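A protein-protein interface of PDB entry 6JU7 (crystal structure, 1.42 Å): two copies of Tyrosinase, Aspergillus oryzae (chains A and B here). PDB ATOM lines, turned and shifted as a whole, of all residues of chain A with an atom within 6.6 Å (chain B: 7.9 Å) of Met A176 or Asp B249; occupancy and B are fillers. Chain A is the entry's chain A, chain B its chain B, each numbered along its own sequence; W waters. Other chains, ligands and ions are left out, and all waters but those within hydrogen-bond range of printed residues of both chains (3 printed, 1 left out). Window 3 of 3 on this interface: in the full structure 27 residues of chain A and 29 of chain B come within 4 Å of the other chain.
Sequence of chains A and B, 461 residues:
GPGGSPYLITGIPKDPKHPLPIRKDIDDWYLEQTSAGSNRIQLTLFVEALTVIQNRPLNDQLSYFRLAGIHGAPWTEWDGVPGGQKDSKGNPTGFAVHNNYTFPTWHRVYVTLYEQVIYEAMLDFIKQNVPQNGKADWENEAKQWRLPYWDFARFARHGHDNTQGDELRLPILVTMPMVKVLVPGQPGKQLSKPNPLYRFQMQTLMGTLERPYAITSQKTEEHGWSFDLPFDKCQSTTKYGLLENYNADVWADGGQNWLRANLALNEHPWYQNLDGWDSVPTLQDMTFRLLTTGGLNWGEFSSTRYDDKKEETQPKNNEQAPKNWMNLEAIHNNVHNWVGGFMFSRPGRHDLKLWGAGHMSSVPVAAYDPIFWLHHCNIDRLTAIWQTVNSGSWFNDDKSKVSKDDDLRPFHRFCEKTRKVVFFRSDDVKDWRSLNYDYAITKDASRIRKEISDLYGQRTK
The side-chain hydroxyl (OH) of Tyr A30 lies within hydrogen-bond range of the side-chain carboxylate (OD2) of Asp B249 (2.6 Å).
The backbone carbonyl oxygen of Tyr A30 is in hydrogen-bond range of the side-chain hydroxyl of Thr A34. The side-chain hydroxyl (OH) of Tyr A30 sits close to the side-chain sulfur (SD) of Met A176, 3.6 Å away. The backbone carbonyl oxygen (O) of Ile A172 sits at hydrogen-bond distance from the side-chain hydroxyl (OG1) of Thr A175 (2.8 Å). ND2 of Asn A195 is in hydrogen-bond range of O of Met A176 (2.8 Å). The backbone carbonyl oxygen (O) of Pro A177 lies within hydrogen-bond range of the backbone NH (N) of Asn A195 (2.9 Å). OD1 of Asn B247 lies within hydrogen-bond range of N of Asp B249, at 2.8 Å.
Among the printed residues, pairs that only touch across the chains: Thr A175 with Val B250 (3.6 Å), Met A176 with Asp B249 (3.8 Å), Pro A177 with Asp B253 (3.5 Å), Trp A258 with Tyr B246 (3.5 Å), Trp A258 with Val B250 (3.7 Å) and Trp A258 with Gly B254 (3.6 Å).
Of the printed residues of chain B, Tyr A30 touches Asp B249 (2.6 Å). Printed residues of chain B within 4 Å of Met A176: Asp B249 (3.8 Å). Lys A180 touches none of the printed residues of chain B. Printed residues of chain B within 4 Å of Trp A258: Tyr B246 (3.5 Å), Val B250 (3.7 Å) and Gly B254 (3.6 Å). Of the printed residues of chain A, Tyr B246 touches Trp A258. Asp B249 touches just these residues of chain A: Tyr A30 and Met A176. Of the printed residues of chain A, Val B250 touches Thr A175 (3.6 Å) and Trp A258 (3.7 Å). Printed residues of chain A within 4 Å of Gly B254: Trp A258. The nearest residue of chain B that does not touch Met A176 is Val B250 (4.3 Å).
Hydrophobic or aromatic side chains of chain A within 4 Å of the printed part of chain B: Tyr A30, Met A176, Pro A177 and Trp A258. Of the 11 printed residues of chain B, 5 touch a printed residue of chain A.
No position is printed for both chains. Of the 7 pairs that touch across the chains among the printed residues, none has its exchanged pair printed and touching as well.
Water W1 bridges NH2 of Arg A40 (2.4 Å) and OD2 of Asp B249 (2.7 Å). Water W2 lies within hydrogen-bond range of the side-chain hydroxyl (OG1) of Thr A34 (2.7 Å), the side-chain amide nitrogen (ND2) of Asn B247 (3.0 Å) and the side-chain carboxylate (OD2) of Asp B249 (3.3 Å). Water W3 bridges O of Asp B249 (3.1 Å) and O of Met A178 (3.3 Å).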
ATOM      1  N   TYR A  30     -11.472 -23.531   4.969  1.00  0.00           N
ATOM      2  CA  TYR A  30     -10.029 -23.522   4.767  1.00  0.00           C
ATOM      3  C   TYR A  30      -9.398 -22.302   5.444  1.00  0.00           C
ATOM      4  O   TYR A  30      -8.375 -22.420   6.123  1.00  0.00           O
ATOM      5  CB  TYR A  30      -9.665 -23.560   3.263  1.00  0.00           C
ATOM      6  CG  TYR A  30      -8.140 -23.604   3.138  1.00  0.00           C
ATOM      7  CD1 TYR A  30      -7.472 -24.774   3.513  1.00  0.00           C
ATOM      8  CD2 TYR A  30      -7.412 -22.516   2.682  1.00  0.00           C
ATOM      9  CE1 TYR A  30      -6.094 -24.859   3.416  1.00  0.00           C
ATOM     10  CE2 TYR A  30      -6.016 -22.600   2.599  1.00  0.00           C
ATOM     11  CZ  TYR A  30      -5.383 -23.765   2.964  1.00  0.00           C
ATOM     12  OH  TYR A  30      -4.007 -23.894   2.915  1.00  0.00           O
ATOM     13  N   THR A  34      -6.730 -22.049   8.652  1.00  0.00           N
ATOM     14  CA  THR A  34      -5.370 -21.634   8.358  1.00  0.00           C
ATOM     15  C   THR A  34      -5.120 -20.156   8.597  1.00  0.00           C
ATOM     16  O   THR A  34      -3.962 -19.725   8.636  1.00  0.00           O
ATOM     17  CB  THR A  34      -4.971 -21.954   6.891  1.00  0.00           C
ATOM     18  OG1 THR A  34      -5.849 -21.251   6.006  1.00  0.00           O
ATOM     19  CG2 THR A  34      -5.090 -23.439   6.581  1.00  0.00           C
ATOM     20  N   ARG A  40      -5.764 -25.974  12.783  1.00  0.00           N
ATOM     21  CA  ARG A  40      -5.705 -26.954  11.719  1.00  0.00           C
ATOM     22  C   ARG A  40      -6.099 -28.374  12.087  1.00  0.00           C
ATOM     23  O   ARG A  40      -5.790 -29.335  11.364  1.00  0.00           O
ATOM     24  CB  ARG A  40      -4.253 -26.971  11.174  1.00  0.00           C
ATOM     25  CG  ARG A  40      -3.950 -25.866  10.196  1.00  0.00           C
ATOM     26  CD  ARG A  40      -2.546 -26.060   9.611  1.00  0.00           C
ATOM     27  NE  ARG A  40      -2.108 -24.801   9.005  1.00  0.00           N
ATOM     28  CZ  ARG A  40      -1.917 -24.589   7.720  1.00  0.00           C
ATOM     29  NH1 ARG A  40      -2.122 -25.538   6.816  1.00  0.00           N
ATOM     30  NH2 ARG A  40      -1.521 -23.389   7.326  1.00  0.00           N
ATOM     31  N   PRO A 171     -12.548 -24.475  -5.322  1.00  0.00           N
ATOM     32  CA  PRO A 171     -12.027 -24.266  -3.966  1.00  0.00           C
ATOM     33  C   PRO A 171     -10.519 -24.070  -3.930  1.00  0.00           C
ATOM     34  O   PRO A 171      -9.757 -24.733  -4.639  1.00  0.00           O
ATOM     35  CB  PRO A 171     -12.366 -25.590  -3.262  1.00  0.00           C
ATOM     36  CG  PRO A 171     -13.553 -26.109  -4.022  1.00  0.00           C
ATOM     37  CD  PRO A 171     -13.321 -25.720  -5.460  1.00  0.00           C
ATOM     38  N   ILE A 172     -10.097 -23.178  -3.035  1.00  0.00           N
ATOM     39  CA  ILE A 172      -8.674 -22.968  -2.774  1.00  0.00           C
ATOM     40  C   ILE A 172      -7.953 -24.302  -2.600  1.00  0.00           C
ATOM     41  O   ILE A 172      -6.949 -24.573  -3.259  1.00  0.00           O
ATOM     42  CB  ILE A 172      -8.461 -22.106  -1.512  1.00  0.00           C
ATOM     43  CG1 ILE A 172      -9.044 -20.696  -1.640  1.00  0.00           C
ATOM     44  CG2 ILE A 172      -7.000 -22.091  -1.115  1.00  0.00           C
ATOM     45  CD1 ILE A 172      -9.341 -20.048  -0.293  1.00  0.00           C
ATOM     46  N   LEU A 173      -8.483 -25.148  -1.716  1.00  0.00           N
ATOM     47  CA  LEU A 173      -7.764 -26.356  -1.332  1.00  0.00           C
ATOM     48  C   LEU A 173      -7.693 -27.333  -2.491  1.00  0.00           C
ATOM     49  O   LEU A 173      -6.731 -28.073  -2.642  1.00  0.00           O
ATOM     50  CB  LEU A 173      -8.473 -26.980  -0.120  1.00  0.00           C
ATOM     51  CG  LEU A 173      -7.811 -28.199   0.506  1.00  0.00           C
ATOM     52  CD1 LEU A 173      -6.358 -27.924   0.855  1.00  0.00           C
ATOM     53  CD2 LEU A 173      -8.584 -28.600   1.760  1.00  0.00           C
ATOM     54  N   VAL A 174      -8.721 -27.332  -3.352  1.00  0.00           N
ATOM     55  CA  VAL A 174      -8.694 -28.246  -4.496  1.00  0.00           C
ATOM     56  C   VAL A 174      -7.574 -27.906  -5.470  1.00  0.00           C
ATOM     57  O   VAL A 174      -7.064 -28.783  -6.173  1.00  0.00           O
ATOM     58  CB  VAL A 174     -10.085 -28.251  -5.167  1.00  0.00           C
ATOM     59  CG1 VAL A 174     -10.009 -28.630  -6.629  1.00  0.00           C
ATOM     60  CG2 VAL A 174     -11.019 -29.181  -4.394  1.00  0.00           C
ATOM     61  N   THR A 175      -7.095 -26.657  -5.493  1.00  0.00           N
ATOM     62  CA  THR A 175      -6.083 -26.238  -6.461  1.00  0.00           C
ATOM     63  C   THR A 175      -4.669 -26.329  -5.893  1.00  0.00           C
ATOM     64  O   THR A 175      -3.738 -25.970  -6.621  1.00  0.00           O
ATOM     65  CB  THR A 175      -6.347 -24.803  -6.961  1.00  0.00           C
ATOM     66  OG1 THR A 175      -6.152 -23.871  -5.879  1.00  0.00           O
ATOM     67  CG2 THR A 175      -7.787 -24.697  -7.413  1.00  0.00           C
ATOM     68  N   MET A 176      -4.486 -26.829  -4.674  1.00  0.00           N
ATOM     69  CA  MET A 176      -3.170 -26.968  -4.038  1.00  0.00           C
ATOM     70  C   MET A 176      -2.641 -28.392  -4.136  1.00  0.00           C
ATOM     71  O   MET A 176      -3.249 -29.348  -3.624  1.00  0.00           O
ATOM     72  CB  MET A 176      -3.304 -26.600  -2.548  1.00  0.00           C
ATOM     73  CG  MET A 176      -3.620 -25.139  -2.295  1.00  0.00           C
ATOM     74  SD  MET A 176      -4.153 -24.794  -0.614  1.00  0.00           S
ATOM     75  CE  MET A 176      -2.877 -25.618   0.326  1.00  0.00           C
ATOM     76  N   PRO A 177      -1.515 -28.624  -4.805  1.00  0.00           N
ATOM     77  CA  PRO A 177      -0.960 -29.984  -4.846  1.00  0.00           C
ATOM     78  C   PRO A 177      -0.541 -30.511  -3.473  1.00  0.00           C
ATOM     79  O   PRO A 177      -0.651 -31.709  -3.206  1.00  0.00           O
ATOM     80  CB  PRO A 177       0.280 -29.812  -5.741  1.00  0.00           C
ATOM     81  CG  PRO A 177       0.069 -28.555  -6.507  1.00  0.00           C
ATOM     82  CD  PRO A 177      -0.778 -27.665  -5.652  1.00  0.00           C
ATOM     83  N   MET A 178      -0.061 -29.648  -2.576  1.00  0.00           N
ATOM     84  CA  MET A 178       0.385 -30.047  -1.232  1.00  0.00           C
ATOM     85  C   MET A 178      -0.385 -29.269  -0.176  1.00  0.00           C
ATOM     86  O   MET A 178      -0.901 -28.178  -0.453  1.00  0.00           O
ATOM     87  CB  MET A 178       1.880 -29.750  -1.090  1.00  0.00           C
ATOM     88  CG  MET A 178       2.749 -30.378  -2.153  1.00  0.00           C
ATOM     89  SD  MET A 178       2.871 -32.164  -2.016  1.00  0.00           S
ATOM     90  CE  MET A 178       3.894 -32.347  -0.551  1.00  0.00           C
ATOM     91  N   VAL A 179      -0.457 -29.803   1.036  1.00  0.00           N
ATOM     92  CA  VAL A 179      -1.204 -29.136   2.101  1.00  0.00           C
ATOM     93  C   VAL A 179      -0.462 -29.347   3.410  1.00  0.00           C
ATOM     94  O   VAL A 179       0.140 -30.394   3.596  1.00  0.00           O
ATOM     95  CB  VAL A 179      -2.642 -29.667   2.189  1.00  0.00           C
ATOM     96  CG1 VAL A 179      -2.662 -31.183   2.365  1.00  0.00           C
ATOM     97  CG2 VAL A 179      -3.380 -28.982   3.338  1.00  0.00           C
ATOM     98  N   LYS A 180      -0.481 -28.354   4.304  1.00  0.00           N
ATOM     99  CA  LYS A 180       0.238 -28.493   5.571  1.00  0.00           C
ATOM    100  C   LYS A 180      -0.705 -28.960   6.670  1.00  0.00           C
ATOM    101  O   LYS A 180      -1.798 -28.423   6.849  1.00  0.00           O
ATOM    102  CB  LYS A 180       0.917 -27.157   5.892  1.00  0.00           C
ATOM    103  N   PRO A 194       1.112 -34.568   0.265  1.00  0.00           N
ATOM    104  CA  PRO A 194       0.267 -34.505  -0.934  1.00  0.00           C
ATOM    105  C   PRO A 194      -1.186 -34.339  -0.535  1.00  0.00           C
ATOM    106  O   PRO A 194      -1.712 -34.936   0.404  1.00  0.00           O
ATOM    107  CB  PRO A 194       0.485 -35.847  -1.605  1.00  0.00           C
ATOM    108  CG  PRO A 194       1.779 -36.360  -1.055  1.00  0.00           C
ATOM    109  CD  PRO A 194       1.912 -35.798   0.339  1.00  0.00           C
ATOM    110  N   ASN A 195      -1.861 -33.463  -1.274  1.00  0.00           N
ATOM    111  CA  ASN A 195      -3.242 -33.143  -0.904  1.00  0.00           C
ATOM    112  C   ASN A 195      -4.236 -34.090  -1.538  1.00  0.00           C
ATOM    113  O   ASN A 195      -4.367 -34.116  -2.771  1.00  0.00           O
ATOM    114  CB  ASN A 195      -3.467 -31.694  -1.343  1.00  0.00           C
ATOM    115  CG  ASN A 195      -4.907 -31.256  -1.145  1.00  0.00           C
ATOM    116  OD1 ASN A 195      -5.709 -31.901  -0.458  1.00  0.00           O
ATOM    117  ND2 ASN A 195      -5.203 -30.131  -1.777  1.00  0.00           N
ATOM    118  N   PRO A 196      -4.963 -34.894  -0.757  1.00  0.00           N
ATOM    119  CA  PRO A 196      -5.842 -35.907  -1.353  1.00  0.00           C
ATOM    120  C   PRO A 196      -7.074 -35.297  -2.005  1.00  0.00           C
ATOM    121  O   PRO A 196      -7.817 -36.041  -2.659  1.00  0.00           O
ATOM    122  CB  PRO A 196      -6.240 -36.782  -0.141  1.00  0.00           C
ATOM    123  CG  PRO A 196      -6.221 -35.806   0.994  1.00  0.00           C
ATOM    124  CD  PRO A 196      -5.011 -34.936   0.719  1.00  0.00           C
ATOM    125  N   LEU A 197      -7.291 -33.988  -1.876  1.00  0.00           N
ATOM    126  CA  LEU A 197      -8.406 -33.331  -2.565  1.00  0.00           C
ATOM    127  C   LEU A 197      -8.012 -32.828  -3.948  1.00  0.00           C
ATOM    128  O   LEU A 197      -8.870 -32.423  -4.735  1.00  0.00           O
ATOM    129  CB  LEU A 197      -8.909 -32.158  -1.712  1.00  0.00           C
ATOM    130  CG  LEU A 197      -9.650 -32.539  -0.420  1.00  0.00           C
ATOM    131  CD1 LEU A 197      -9.854 -31.307   0.461  1.00  0.00           C
ATOM    132  CD2 LEU A 197     -10.969 -33.230  -0.716  1.00  0.00           C
ATOM    133  N   TYR A 198      -6.726 -32.820  -4.268  1.00  0.00           N
ATOM    134  CA  TYR A 198      -6.236 -32.250  -5.524  1.00  0.00           C
ATOM    135  C   TYR A 198      -6.541 -33.132  -6.731  1.00  0.00           C
ATOM    136  O   TYR A 198      -6.805 -32.610  -7.809  1.00  0.00           O
ATOM    137  CB  TYR A 198      -4.731 -32.060  -5.389  1.00  0.00           C
ATOM    138  CG  TYR A 198      -3.966 -31.439  -6.532  1.00  0.00           C
ATOM    139  CD1 TYR A 198      -4.179 -30.112  -6.925  1.00  0.00           C
ATOM    140  CD2 TYR A 198      -2.975 -32.164  -7.194  1.00  0.00           C
ATOM    141  CE1 TYR A 198      -3.452 -29.556  -7.967  1.00  0.00           C
ATOM    142  CE2 TYR A 198      -2.241 -31.607  -8.230  1.00  0.00           C
ATOM    143  CZ  TYR A 198      -2.481 -30.304  -8.610  1.00  0.00           C
ATOM    144  OH  TYR A 198      -1.739 -29.756  -9.639  1.00  0.00           O
ATOM    145  N   TRP A 258      -6.833 -25.989 -13.408  1.00  0.00           N
ATOM    146  CA  TRP A 258      -7.872 -25.287 -12.667  1.00  0.00           C
ATOM    147  C   TRP A 258      -8.138 -23.903 -13.238  1.00  0.00           C
ATOM    148  O   TRP A 258      -9.227 -23.357 -13.026  1.00  0.00           O
ATOM    149  CB  TRP A 258      -7.518 -25.210 -11.181  1.00  0.00           C
ATOM    150  CG  TRP A 258      -6.227 -24.578 -10.788  1.00  0.00           C
ATOM    151  CD1 TRP A 258      -4.999 -25.162 -10.580  1.00  0.00           C
ATOM    152  CD2 TRP A 258      -6.040 -23.176 -10.530  1.00  0.00           C
ATOM    153  NE1 TRP A 258      -4.076 -24.211 -10.219  1.00  0.00           N
ATOM    154  CE2 TRP A 258      -4.681 -22.991 -10.177  1.00  0.00           C
ATOM    155  CE3 TRP A 258      -6.889 -22.073 -10.550  1.00  0.00           C
ATOM    156  CZ2 TRP A 258      -4.161 -21.732  -9.863  1.00  0.00           C
ATOM    157  CZ3 TRP A 258      -6.371 -20.827 -10.241  1.00  0.00           C
ATOM    158  CH2 TRP A 258      -5.014 -20.663  -9.897  1.00  0.00           C
ATOM    159  N   LEU B 205       9.558 -22.513   0.771  1.00  0.00           N
ATOM    160  CA  LEU B 205       9.290 -21.375  -0.104  1.00  0.00           C
ATOM    161  C   LEU B 205      10.614 -20.713  -0.481  1.00  0.00           C
ATOM    162  O   LEU B 205      11.516 -20.558   0.356  1.00  0.00           O
ATOM    163  CB  LEU B 205       8.382 -20.372   0.590  1.00  0.00           C
ATOM    164  CG  LEU B 205       7.011 -20.890   1.037  1.00  0.00           C
ATOM    165  CD1 LEU B 205       6.198 -19.734   1.593  1.00  0.00           C
ATOM    166  CD2 LEU B 205       6.263 -21.567  -0.110  1.00  0.00           C
ATOM    167  N   LYS B 233       7.077 -16.410  -2.566  1.00  0.00           N
ATOM    168  CA  LYS B 233       6.031 -17.213  -1.961  1.00  0.00           C
ATOM    169  C   LYS B 233       5.859 -18.526  -2.707  1.00  0.00           C
ATOM    170  O   LYS B 233       4.980 -19.312  -2.376  1.00  0.00           O
ATOM    171  CB  LYS B 233       4.704 -16.440  -1.943  1.00  0.00           C
ATOM    172  CG  LYS B 233       4.800 -15.012  -1.431  1.00  0.00           C
ATOM    173  CD  LYS B 233       4.793 -14.972   0.080  1.00  0.00           C
ATOM    174  CE  LYS B 233       4.758 -13.547   0.628  1.00  0.00           C
ATOM    175  NZ  LYS B 233       5.289 -13.477   2.020  1.00  0.00           N
ATOM    176  N   TYR B 246      -5.508 -14.307  -5.068  1.00  0.00           N
ATOM    177  CA  TYR B 246      -5.546 -15.716  -4.705  1.00  0.00           C
ATOM    178  C   TYR B 246      -4.714 -15.964  -3.448  1.00  0.00           C
ATOM    179  O   TYR B 246      -3.656 -15.373  -3.225  1.00  0.00           O
ATOM    180  CB  TYR B 246      -5.016 -16.593  -5.864  1.00  0.00           C
ATOM    181  CG  TYR B 246      -6.062 -16.801  -6.942  1.00  0.00           C
ATOM    182  CD1 TYR B 246      -6.616 -18.049  -7.181  1.00  0.00           C
ATOM    183  CD2 TYR B 246      -6.534 -15.739  -7.716  1.00  0.00           C
ATOM    184  CE1 TYR B 246      -7.570 -18.235  -8.150  1.00  0.00           C
ATOM    185  CE2 TYR B 246      -7.509 -15.922  -8.696  1.00  0.00           C
ATOM    186  CZ  TYR B 246      -8.025 -17.175  -8.912  1.00  0.00           C
ATOM    187  OH  TYR B 246      -8.992 -17.428  -9.863  1.00  0.00           O
ATOM    188  N   ASN B 247      -5.226 -16.881  -2.619  1.00  0.00           N
ATOM    189  CA  ASN B 247      -4.562 -17.267  -1.376  1.00  0.00           C
ATOM    190  C   ASN B 247      -3.129 -17.683  -1.664  1.00  0.00           C
ATOM    191  O   ASN B 247      -2.874 -18.409  -2.628  1.00  0.00           O
ATOM    192  CB  ASN B 247      -5.350 -18.428  -0.760  1.00  0.00           C
ATOM    193  CG  ASN B 247      -4.858 -18.858   0.605  1.00  0.00           C
ATOM    194  OD1 ASN B 247      -3.770 -19.420   0.742  1.00  0.00           O
ATOM    195  ND2 ASN B 247      -5.680 -18.599   1.629  1.00  0.00           N
ATOM    196  N   ALA B 248      -2.189 -17.206  -0.853  1.00  0.00           N
ATOM    197  CA  ALA B 248      -0.771 -17.457  -1.106  1.00  0.00           C
ATOM    198  C   ALA B 248      -0.432 -18.938  -1.021  1.00  0.00           C
ATOM    199  O   ALA B 248       0.643 -19.318  -1.510  1.00  0.00           O
ATOM    200  CB  ALA B 248       0.105 -16.644  -0.159  1.00  0.00           C
ATOM    201  N   ASP B 249      -1.312 -19.767  -0.450  1.00  0.00           N
ATOM    202  CA  ASP B 249      -1.030 -21.206  -0.451  1.00  0.00           C
ATOM    203  C   ASP B 249      -1.186 -21.804  -1.840  1.00  0.00           C
ATOM    204  O   ASP B 249      -0.590 -22.847  -2.144  1.00  0.00           O
ATOM    205  CB  ASP B 249      -1.910 -21.951   0.552  1.00  0.00           C
ATOM    206  CG  ASP B 249      -1.616 -21.521   1.981  1.00  0.00           C
ATOM    207  OD1 ASP B 249      -0.546 -20.907   2.219  1.00  0.00           O
ATOM    208  OD2 ASP B 249      -2.433 -21.776   2.884  1.00  0.00           O
ATOM    209  N   VAL B 250      -1.939 -21.118  -2.709  1.00  0.00           N
ATOM    210  CA  VAL B 250      -1.962 -21.554  -4.108  1.00  0.00           C
ATOM    211  C   VAL B 250      -0.642 -21.221  -4.787  1.00  0.00           C
ATOM    212  O   VAL B 250      -0.095 -22.005  -5.567  1.00  0.00           O
ATOM    213  CB  VAL B 250      -3.132 -20.877  -4.845  1.00  0.00           C
ATOM    214  CG1 VAL B 250      -3.135 -21.255  -6.317  1.00  0.00           C
ATOM    215  CG2 VAL B 250      -4.476 -21.208  -4.207  1.00  0.00           C
ATOM    216  N   TRP B 251      -0.085 -20.059  -4.479  1.00  0.00           N
ATOM    217  CA  TRP B 251       1.180 -19.577  -5.044  1.00  0.00           C
ATOM    218  C   TRP B 251       2.356 -20.479  -4.718  1.00  0.00           C
ATOM    219  O   TRP B 251       3.316 -20.530  -5.501  1.00  0.00           O
ATOM    220  CB  TRP B 251       1.492 -18.166  -4.557  1.00  0.00           C
ATOM    221  CG  TRP B 251       0.519 -17.116  -4.995  1.00  0.00           C
ATOM    222  CD1 TRP B 251      -0.466 -17.176  -5.947  1.00  0.00           C
ATOM    223  CD2 TRP B 251       0.473 -15.794  -4.437  1.00  0.00           C
ATOM    224  NE1 TRP B 251      -1.109 -15.969  -6.018  1.00  0.00           N
ATOM    225  CE2 TRP B 251      -0.557 -15.107  -5.098  1.00  0.00           C
ATOM    226  CE3 TRP B 251       1.230 -15.158  -3.435  1.00  0.00           C
ATOM    227  CZ2 TRP B 251      -0.860 -13.785  -4.786  1.00  0.00           C
ATOM    228  CZ3 TRP B 251       0.920 -13.841  -3.125  1.00  0.00           C
ATOM    229  CH2 TRP B 251      -0.115 -13.180  -3.802  1.00  0.00           C
ATOM    230  N   ALA B 252       2.243 -21.218  -3.627  1.00  0.00           N
ATOM    231  CA  ALA B 252       3.351 -22.121  -3.281  1.00  0.00           C
ATOM    232  C   ALA B 252       3.682 -23.048  -4.435  1.00  0.00           C
ATOM    233  O   ALA B 252       4.846 -23.367  -4.734  1.00  0.00           O
ATOM    234  CB  ALA B 252       2.996 -22.899  -2.020  1.00  0.00           C
ATOM    235  N   ASP B 253       2.632 -23.537  -5.079  1.00  0.00           N
ATOM    236  CA  ASP B 253       2.817 -24.320  -6.295  1.00  0.00           C
ATOM    237  C   ASP B 253       1.596 -24.097  -7.192  1.00  0.00           C
ATOM    238  O   ASP B 253       0.574 -24.740  -7.002  1.00  0.00           O
ATOM    239  CB  ASP B 253       3.018 -25.794  -5.986  1.00  0.00           C
ATOM    240  CG  ASP B 253       3.270 -26.634  -7.215  1.00  0.00           C
ATOM    241  OD1 ASP B 253       3.039 -26.155  -8.338  1.00  0.00           O
ATOM    242  OD2 ASP B 253       3.664 -27.811  -7.057  1.00  0.00           O
ATOM    243  N   GLY B 254       1.692 -23.150  -8.104  1.00  0.00           N
ATOM    244  CA  GLY B 254       0.541 -22.758  -8.900  1.00  0.00           C
ATOM    245  C   GLY B 254       0.332 -23.603 -10.136  1.00  0.00           C
ATOM    246  O   GLY B 254      -0.618 -23.352 -10.890  1.00  0.00           O
HETATM  247  O   HOH W   1      -1.242 -22.112   5.265  1.00  0.00           O
HETATM  248  O   HOH W   2      -4.659 -19.708   4.174  1.00  0.00           O
HETATM  249  O   HOH W   3       0.488 -25.225  -0.487  1.00  0.00           O
